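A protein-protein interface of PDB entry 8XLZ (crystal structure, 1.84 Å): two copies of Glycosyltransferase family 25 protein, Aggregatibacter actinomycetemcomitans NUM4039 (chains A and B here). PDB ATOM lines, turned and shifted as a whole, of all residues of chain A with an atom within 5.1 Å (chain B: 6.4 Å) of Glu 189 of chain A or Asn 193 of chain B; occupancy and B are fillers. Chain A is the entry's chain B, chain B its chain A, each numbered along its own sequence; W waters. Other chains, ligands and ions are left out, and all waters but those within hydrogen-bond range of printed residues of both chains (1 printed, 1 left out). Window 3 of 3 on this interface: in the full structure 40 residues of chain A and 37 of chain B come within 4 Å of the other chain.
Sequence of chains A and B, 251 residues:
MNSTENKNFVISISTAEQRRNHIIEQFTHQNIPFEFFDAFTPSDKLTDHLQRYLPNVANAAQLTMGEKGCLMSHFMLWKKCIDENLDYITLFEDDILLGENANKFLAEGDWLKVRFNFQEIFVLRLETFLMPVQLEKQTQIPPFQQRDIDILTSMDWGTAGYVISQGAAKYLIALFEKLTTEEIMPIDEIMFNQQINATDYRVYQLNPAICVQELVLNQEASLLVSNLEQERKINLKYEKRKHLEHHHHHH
Glu 189 of chain A touches Asn 193 of chain B, but with the chains exchanged Asn 193 of chain A does not touch Glu 189 of chain B (5.5 Å).
Positions printed for both chains: 188, 189, 190, 191, 192, 193 and 194.
Of the printed residues of chain B, Glu 189 of chain A touches Asn 193 (2.8 Å).
Of the printed residues of chain B, Leu 152 of chain A touches Trp 157 (3.98 Å) and Val 203 (2.9 Å).
Of the printed residues of chain B, Met 155 of chain A touches Trp 157 and Asn 193.
Of the printed residues of chain A, Val 203 of chain B touches Leu 152.
The nearest printed residue of chain B that does not touch Glu 189 of chain A is Glu 189 of chain B (4.7 Å).
The nearest printed residue of chain A that does not touch Asn 193 of chain B is Leu 152 of chain A (4.9 Å).
The side-chain carboxylate (OD2) of Asp 188 of chain B lies within hydrogen-bond range of the backbone NH (N) of Trp 157 of chain B (3.0 Å).
ND2 of Asn 193 of chain B lies within hydrogen-bond range of OE2 of Glu 189 of chain B (2.7 Å).
O of Glu 189 of chain A is in hydrogen-bond range of ND2 of Asn 193 of chain A, at 3.2 Å.
Among the printed residues, pairs that only touch across the chains: Leu 152 of chain A with Trp 157 of chain B (3.98 Å), Met 155 of chain A with Trp 157 of chain B (3.8 Å) and Met 155 of chain A with Asn 193 of chain B (3.5 Å).
The side-chain amide nitrogen (ND2) of Asn 193 of chain B is in hydrogen-bond range of the side-chain carboxylate (OE2) of Glu 189 of chain A, 2.8 Å away.
The backbone carbonyl oxygen of Val 203 of chain B is in hydrogen-bond range of the backbone NH of Leu 152 of chain A, 2.9 Å away.
Of the 12 printed residues of chain B, 3 touch a printed residue of chain A.
Printed residues of chain B that touch a printed residue of chain A: Trp 157, Asn 193 and Val 203.
Hydrophobic or aromatic side chains of chain B within 4 Å of the printed part of chain A: Trp 157.
Among the printed residues, no Asp or Glu carboxylate lies within 4 Å of a Lys or Arg side-chain nitrogen of the other chain.
Water W1 lies within hydrogen-bond range of the side-chain amide oxygen of Asn 193 of chain B (2.9 Å) and the backbone NH of Met 155 of chain A (3.0 Å).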
ATOM      1  N   LEU A 152       3.875 -31.959   7.198  1.00  0.00           N
ATOM      2  CA  LEU A 152       3.011 -30.775   7.178  1.00  0.00           C
ATOM      3  C   LEU A 152       1.630 -31.114   6.623  1.00  0.00           C
ATOM      4  O   LEU A 152       1.524 -31.597   5.499  1.00  0.00           O
ATOM      5  CB  LEU A 152       3.624 -29.691   6.305  1.00  0.00           C
ATOM      6  CG  LEU A 152       2.824 -28.399   6.173  1.00  0.00           C
ATOM      7  CD1 LEU A 152       2.829 -27.655   7.511  1.00  0.00           C
ATOM      8  CD2 LEU A 152       3.359 -27.554   5.012  1.00  0.00           C
ATOM      9  N   MET A 155      -1.659 -25.086   7.471  1.00  0.00           N
ATOM     10  CA  MET A 155      -1.308 -23.860   8.155  1.00  0.00           C
ATOM     11  C   MET A 155      -2.507 -23.522   9.036  1.00  0.00           C
ATOM     12  O   MET A 155      -3.595 -23.307   8.548  1.00  0.00           O
ATOM     13  CB  MET A 155      -1.085 -22.710   7.161  1.00  0.00           C
ATOM     14  CG  MET A 155      -0.247 -23.041   5.930  1.00  0.00           C
ATOM     15  SD  MET A 155       1.481 -23.366   6.279  1.00  0.00           S
ATOM     16  CE  MET A 155       1.971 -21.733   6.806  1.00  0.00           C
ATOM     17  N   MET A 185     -11.220 -20.411   1.799  1.00  0.00           N
ATOM     18  CA  MET A 185     -10.322 -21.255   2.571  1.00  0.00           C
ATOM     19  C   MET A 185     -10.915 -21.281   3.975  1.00  0.00           C
ATOM     20  O   MET A 185     -11.848 -20.518   4.257  1.00  0.00           O
ATOM     21  CB  MET A 185      -8.925 -20.637   2.619  1.00  0.00           C
ATOM     22  CG  MET A 185      -8.172 -20.591   1.299  1.00  0.00           C
ATOM     23  SD  MET A 185      -6.588 -19.733   1.452  1.00  0.00           S
ATOM     24  CE  MET A 185      -7.177 -18.078   1.664  1.00  0.00           C
ATOM     25  N   PRO A 186     -10.384 -22.134   4.872  1.00  0.00           N
ATOM     26  CA  PRO A 186     -10.868 -22.106   6.256  1.00  0.00           C
ATOM     27  C   PRO A 186     -10.851 -20.687   6.837  1.00  0.00           C
ATOM     28  O   PRO A 186     -10.009 -19.886   6.457  1.00  0.00           O
ATOM     29  CB  PRO A 186      -9.899 -23.030   6.993  1.00  0.00           C
ATOM     30  CG  PRO A 186      -9.392 -23.987   5.933  1.00  0.00           C
ATOM     31  CD  PRO A 186      -9.424 -23.226   4.628  1.00  0.00           C
ATOM     32  N   ILE A 187     -11.784 -20.377   7.726  1.00  0.00           N
ATOM     33  CA  ILE A 187     -11.892 -19.021   8.269  1.00  0.00           C
ATOM     34  C   ILE A 187     -10.580 -18.458   8.833  1.00  0.00           C
ATOM     35  O   ILE A 187     -10.246 -17.290   8.657  1.00  0.00           O
ATOM     36  CB  ILE A 187     -13.000 -18.942   9.338  1.00  0.00           C
ATOM     37  CG1 ILE A 187     -13.187 -17.495   9.762  1.00  0.00           C
ATOM     38  CG2 ILE A 187     -12.733 -19.865  10.549  1.00  0.00           C
ATOM     39  CD1 ILE A 187     -14.484 -17.271  10.506  1.00  0.00           C
ATOM     40  N   ASP A 188      -9.839 -19.301   9.524  1.00  0.00           N
ATOM     41  CA  ASP A 188      -8.580 -18.897  10.123  1.00  0.00           C
ATOM     42  C   ASP A 188      -7.539 -18.520   9.087  1.00  0.00           C
ATOM     43  O   ASP A 188      -6.760 -17.596   9.302  1.00  0.00           O
ATOM     44  CB  ASP A 188      -8.061 -19.994  11.029  1.00  0.00           C
ATOM     45  CG  ASP A 188      -7.758 -21.298  10.303  1.00  0.00           C
ATOM     46  OD1 ASP A 188      -8.624 -21.875   9.641  1.00  0.00           O
ATOM     47  OD2 ASP A 188      -6.639 -21.787  10.465  1.00  0.00           O
ATOM     48  N   GLU A 189      -7.541 -19.200   7.953  1.00  0.00           N
ATOM     49  CA  GLU A 189      -6.592 -18.897   6.878  1.00  0.00           C
ATOM     50  C   GLU A 189      -6.999 -17.606   6.203  1.00  0.00           C
ATOM     51  O   GLU A 189      -6.160 -16.792   5.887  1.00  0.00           O
ATOM     52  CB  GLU A 189      -6.479 -20.017   5.827  1.00  0.00           C
ATOM     53  CG  GLU A 189      -5.370 -19.717   4.809  1.00  0.00           C
ATOM     54  CD  GLU A 189      -4.914 -20.905   3.989  1.00  0.00           C
ATOM     55  OE1 GLU A 189      -5.780 -21.604   3.429  1.00  0.00           O
ATOM     56  OE2 GLU A 189      -3.683 -21.115   3.884  1.00  0.00           O
ATOM     57  N   ILE A 190      -8.303 -17.407   6.003  1.00  0.00           N
ATOM     58  CA  ILE A 190      -8.778 -16.148   5.424  1.00  0.00           C
ATOM     59  C   ILE A 190      -8.436 -14.988   6.331  1.00  0.00           C
ATOM     60  O   ILE A 190      -7.981 -13.941   5.861  1.00  0.00           O
ATOM     61  CB  ILE A 190     -10.302 -16.132   5.152  1.00  0.00           C
ATOM     62  CG1 ILE A 190     -10.671 -17.184   4.114  1.00  0.00           C
ATOM     63  CG2 ILE A 190     -10.776 -14.754   4.686  1.00  0.00           C
ATOM     64  CD1 ILE A 190     -10.079 -16.945   2.733  1.00  0.00           C
ATOM     65  N   MET A 191      -8.608 -15.169   7.634  1.00  0.00           N
ATOM     66  CA  MET A 191      -8.340 -14.059   8.541  1.00  0.00           C
ATOM     67  C   MET A 191      -6.835 -13.827   8.668  1.00  0.00           C
ATOM     68  O   MET A 191      -6.391 -12.687   8.699  1.00  0.00           O
ATOM     69  CB  MET A 191      -8.999 -14.273   9.891  1.00  0.00           C
ATOM     70  CG  MET A 191     -10.513 -14.174   9.787  1.00  0.00           C
ATOM     71  SD  MET A 191     -11.373 -14.414  11.329  1.00  0.00           S
ATOM     72  CE  MET A 191     -10.960 -12.911  12.214  1.00  0.00           C
ATOM     73  N   PHE A 192      -6.058 -14.900   8.748  1.00  0.00           N
ATOM     74  CA  PHE A 192      -4.582 -14.784   8.729  1.00  0.00           C
ATOM     75  C   PHE A 192      -4.048 -13.993   7.532  1.00  0.00           C
ATOM     76  O   PHE A 192      -3.187 -13.131   7.690  1.00  0.00           O
ATOM     77  CB  PHE A 192      -3.899 -16.155   8.695  1.00  0.00           C
ATOM     78  CG  PHE A 192      -2.430 -16.080   8.925  1.00  0.00           C
ATOM     79  CD1 PHE A 192      -1.951 -15.867  10.202  1.00  0.00           C
ATOM     80  CD2 PHE A 192      -1.520 -16.213   7.869  1.00  0.00           C
ATOM     81  CE1 PHE A 192      -0.595 -15.789  10.447  1.00  0.00           C
ATOM     82  CE2 PHE A 192      -0.157 -16.108   8.096  1.00  0.00           C
ATOM     83  CZ  PHE A 192       0.305 -15.901   9.394  1.00  0.00           C
ATOM     84  N   ASN A 193      -4.561 -14.297   6.349  1.00  0.00           N
ATOM     85  CA  ASN A 193      -4.175 -13.593   5.125  1.00  0.00           C
ATOM     86  C   ASN A 193      -4.642 -12.137   5.050  1.00  0.00           C
ATOM     87  O   ASN A 193      -4.085 -11.391   4.282  1.00  0.00           O
ATOM     88  CB  ASN A 193      -4.616 -14.383   3.876  1.00  0.00           C
ATOM     89  CG  ASN A 193      -3.860 -15.700   3.726  1.00  0.00           C
ATOM     90  OD1 ASN A 193      -2.726 -15.799   4.128  1.00  0.00           O
ATOM     91  ND2 ASN A 193      -4.506 -16.719   3.178  1.00  0.00           N
ATOM     92  N   GLN A 194      -5.661 -11.744   5.818  1.00  0.00           N
ATOM     93  CA  GLN A 194      -6.058 -10.356   5.925  1.00  0.00           C
ATOM     94  C   GLN A 194      -5.150  -9.495   6.802  1.00  0.00           C
ATOM     95  O   GLN A 194      -5.295  -8.273   6.803  1.00  0.00           O
ATOM     96  CB  GLN A 194      -7.485 -10.249   6.472  1.00  0.00           C
ATOM     97  CG  GLN A 194      -8.543 -10.639   5.453  1.00  0.00           C
ATOM     98  CD  GLN A 194      -8.491  -9.762   4.198  1.00  0.00           C
ATOM     99  OE1 GLN A 194      -8.766  -8.550   4.251  1.00  0.00           O
ATOM    100  NE2 GLN A 194      -8.141 -10.367   3.075  1.00  0.00           N
ATOM    101  N   TRP B 157       5.868 -17.389   5.008  1.00  0.00           N
ATOM    102  CA  TRP B 157       6.517 -18.438   5.789  1.00  0.00           C
ATOM    103  C   TRP B 157       7.929 -18.675   5.251  1.00  0.00           C
ATOM    104  O   TRP B 157       8.226 -18.360   4.091  1.00  0.00           O
ATOM    105  CB  TRP B 157       5.714 -19.714   5.720  1.00  0.00           C
ATOM    106  CG  TRP B 157       5.914 -20.681   6.853  1.00  0.00           C
ATOM    107  CD1 TRP B 157       6.156 -20.395   8.175  1.00  0.00           C
ATOM    108  CD2 TRP B 157       5.793 -22.100   6.774  1.00  0.00           C
ATOM    109  NE1 TRP B 157       6.218 -21.553   8.911  1.00  0.00           N
ATOM    110  CE2 TRP B 157       5.979 -22.615   8.081  1.00  0.00           C
ATOM    111  CE3 TRP B 157       5.538 -22.993   5.726  1.00  0.00           C
ATOM    112  CZ2 TRP B 157       5.937 -23.979   8.356  1.00  0.00           C
ATOM    113  CZ3 TRP B 157       5.497 -24.346   6.001  1.00  0.00           C
ATOM    114  CH2 TRP B 157       5.678 -24.827   7.309  1.00  0.00           C
ATOM    115  N   ASP B 188       6.970 -19.525  -0.838  1.00  0.00           N
ATOM    116  CA  ASP B 188       6.600 -20.358   0.295  1.00  0.00           C
ATOM    117  C   ASP B 188       5.214 -20.989   0.100  1.00  0.00           C
ATOM    118  O   ASP B 188       4.971 -22.157   0.465  1.00  0.00           O
ATOM    119  CB  ASP B 188       6.622 -19.552   1.588  1.00  0.00           C
ATOM    120  CG  ASP B 188       5.606 -18.388   1.588  1.00  0.00           C
ATOM    121  OD1 ASP B 188       5.791 -17.482   0.745  1.00  0.00           O
ATOM    122  OD2 ASP B 188       4.657 -18.382   2.430  1.00  0.00           O
ATOM    123  N   GLU B 189       4.312 -20.213  -0.509  1.00  0.00           N
ATOM    124  CA  GLU B 189       2.942 -20.645  -0.716  1.00  0.00           C
ATOM    125  C   GLU B 189       2.939 -21.740  -1.789  1.00  0.00           C
ATOM    126  O   GLU B 189       2.238 -22.749  -1.677  1.00  0.00           O
ATOM    127  CB  GLU B 189       2.088 -19.430  -1.119  1.00  0.00           C
ATOM    128  CG  GLU B 189       0.605 -19.660  -1.290  1.00  0.00           C
ATOM    129  CD  GLU B 189      -0.180 -19.855   0.014  1.00  0.00           C
ATOM    130  OE1 GLU B 189       0.143 -19.283   1.072  1.00  0.00           O
ATOM    131  OE2 GLU B 189      -1.170 -20.596  -0.033  1.00  0.00           O
ATOM    132  N   ILE B 190       3.745 -21.556  -2.822  1.00  0.00           N
ATOM    133  CA  ILE B 190       3.828 -22.563  -3.883  1.00  0.00           C
ATOM    134  C   ILE B 190       4.483 -23.846  -3.331  1.00  0.00           C
ATOM    135  O   ILE B 190       4.040 -24.931  -3.604  1.00  0.00           O
ATOM    136  CB  ILE B 190       4.612 -22.066  -5.105  1.00  0.00           C
ATOM    137  CG1 ILE B 190       3.942 -20.820  -5.741  1.00  0.00           C
ATOM    138  CG2 ILE B 190       4.736 -23.180  -6.133  1.00  0.00           C
ATOM    139  CD1 ILE B 190       2.545 -21.065  -6.282  1.00  0.00           C
ATOM    140  N   MET B 191       5.560 -23.712  -2.584  1.00  0.00           N
ATOM    141  CA  MET B 191       6.293 -24.879  -2.161  1.00  0.00           C
ATOM    142  C   MET B 191       5.566 -25.660  -1.077  1.00  0.00           C
ATOM    143  O   MET B 191       5.682 -26.884  -1.038  1.00  0.00           O
ATOM    144  CB  MET B 191       7.673 -24.497  -1.603  1.00  0.00           C
ATOM    145  CG  MET B 191       8.651 -24.026  -2.621  1.00  0.00           C
ATOM    146  SD  MET B 191      10.177 -23.669  -1.757  1.00  0.00           S
ATOM    147  CE  MET B 191      10.637 -25.313  -1.220  1.00  0.00           C
ATOM    148  N   PHE B 192       4.907 -24.971  -0.153  1.00  0.00           N
ATOM    149  CA  PHE B 192       4.462 -25.660   1.043  1.00  0.00           C
ATOM    150  C   PHE B 192       2.941 -25.790   1.038  1.00  0.00           C
ATOM    151  O   PHE B 192       2.415 -26.898   0.821  1.00  0.00           O
ATOM    152  CB  PHE B 192       5.037 -24.979   2.272  1.00  0.00           C
ATOM    153  CG  PHE B 192       6.540 -24.985   2.313  1.00  0.00           C
ATOM    154  CD1 PHE B 192       7.256 -26.158   2.107  1.00  0.00           C
ATOM    155  CD2 PHE B 192       7.237 -23.826   2.591  1.00  0.00           C
ATOM    156  CE1 PHE B 192       8.646 -26.164   2.167  1.00  0.00           C
ATOM    157  CE2 PHE B 192       8.637 -23.832   2.674  1.00  0.00           C
ATOM    158  CZ  PHE B 192       9.340 -24.995   2.438  1.00  0.00           C
ATOM    159  N   ASN B 193       2.259 -24.668   1.199  1.00  0.00           N
ATOM    160  CA  ASN B 193       0.807 -24.655   1.345  1.00  0.00           C
ATOM    161  C   ASN B 193       0.006 -25.315   0.218  1.00  0.00           C
ATOM    162  O   ASN B 193      -0.856 -26.176   0.477  1.00  0.00           O
ATOM    163  CB  ASN B 193       0.304 -23.221   1.537  1.00  0.00           C
ATOM    164  CG  ASN B 193      -1.034 -23.170   2.266  1.00  0.00           C
ATOM    165  OD1 ASN B 193      -1.474 -24.160   2.865  1.00  0.00           O
ATOM    166  ND2 ASN B 193      -1.685 -22.018   2.224  1.00  0.00           N
ATOM    167  N   GLN B 194       0.316 -24.961  -1.024  1.00  0.00           N
ATOM    168  CA  GLN B 194      -0.459 -25.465  -2.172  1.00  0.00           C
ATOM    169  C   GLN B 194      -0.268 -26.957  -2.456  1.00  0.00           C
ATOM    170  O   GLN B 194      -1.062 -27.546  -3.184  1.00  0.00           O
ATOM    171  CB  GLN B 194      -0.134 -24.707  -3.463  1.00  0.00           C
ATOM    172  CG  GLN B 194      -0.425 -23.223  -3.449  1.00  0.00           C
ATOM    173  CD  GLN B 194      -1.850 -22.882  -3.038  1.00  0.00           C
ATOM    174  OE1 GLN B 194      -2.064 -22.147  -2.069  1.00  0.00           O
ATOM    175  NE2 GLN B 194      -2.830 -23.413  -3.765  1.00  0.00           N
ATOM    176  N   GLN B 195       0.794 -27.553  -1.908  1.00  0.00           N
ATOM    177  CA  GLN B 195       1.108 -28.945  -2.169  1.00  0.00           C
ATOM    178  C   GLN B 195       0.695 -29.877  -1.025  1.00  0.00           C
ATOM    179  O   GLN B 195       1.087 -31.047  -1.045  1.00  0.00           O
ATOM    180  CB  GLN B 195       2.631 -29.111  -2.419  1.00  0.00           C
ATOM    181  CG  GLN B 195       3.244 -28.127  -3.422  1.00  0.00           C
ATOM    182  CD  GLN B 195       2.467 -28.072  -4.721  1.00  0.00           C
ATOM    183  OE1 GLN B 195       2.089 -29.097  -5.261  1.00  0.00           O
ATOM    184  NE2 GLN B 195       2.222 -26.865  -5.223  1.00  0.00           N
ATOM    185  N   ILE B 196      -0.072 -29.384  -0.044  1.00  0.00           N
ATOM    186  CA  ILE B 196      -0.442 -30.199   1.126  1.00  0.00           C
ATOM    187  C   ILE B 196      -1.262 -31.445   0.735  1.00  0.00           C
ATOM    188  O   ILE B 196      -1.024 -32.542   1.253  1.00  0.00           O
ATOM    189  CB  ILE B 196      -1.119 -29.317   2.214  1.00  0.00           C
ATOM    190  CG1 ILE B 196      -0.035 -28.625   3.049  1.00  0.00           C
ATOM    191  CG2 ILE B 196      -2.022 -30.135   3.132  1.00  0.00           C
ATOM    192  CD1 ILE B 196      -0.486 -27.356   3.737  1.00  0.00           C
ATOM    193  N   ASN B 197      -2.184 -31.291  -0.215  1.00  0.00           N
ATOM    194  CA  ASN B 197      -2.934 -32.445  -0.751  1.00  0.00           C
ATOM    195  C   ASN B 197      -2.501 -32.939  -2.125  1.00  0.00           C
ATOM    196  O   ASN B 197      -3.309 -33.554  -2.827  1.00  0.00           O
ATOM    197  CB  ASN B 197      -4.436 -32.129  -0.816  1.00  0.00           C
ATOM    198  CG  ASN B 197      -5.010 -31.803   0.540  1.00  0.00           C
ATOM    199  OD1 ASN B 197      -4.893 -32.587   1.486  1.00  0.00           O
ATOM    200  ND2 ASN B 197      -5.633 -30.640   0.649  1.00  0.00           N
ATOM    201  N   VAL B 203       5.679 -32.657   2.132  1.00  0.00           N
ATOM    202  CA  VAL B 203       6.502 -31.734   2.847  1.00  0.00           C
ATOM    203  C   VAL B 203       6.698 -32.305   4.232  1.00  0.00           C
ATOM    204  O   VAL B 203       5.735 -32.454   4.986  1.00  0.00           O
ATOM    205  CB  VAL B 203       5.840 -30.362   2.945  1.00  0.00           C
ATOM    206  CG1 VAL B 203       6.719 -29.419   3.762  1.00  0.00           C
ATOM    207  CG2 VAL B 203       5.605 -29.818   1.532  1.00  0.00           C
HETATM  208  O   HOH W   1      -3.351 -24.725   5.041  1.00  0.00           O
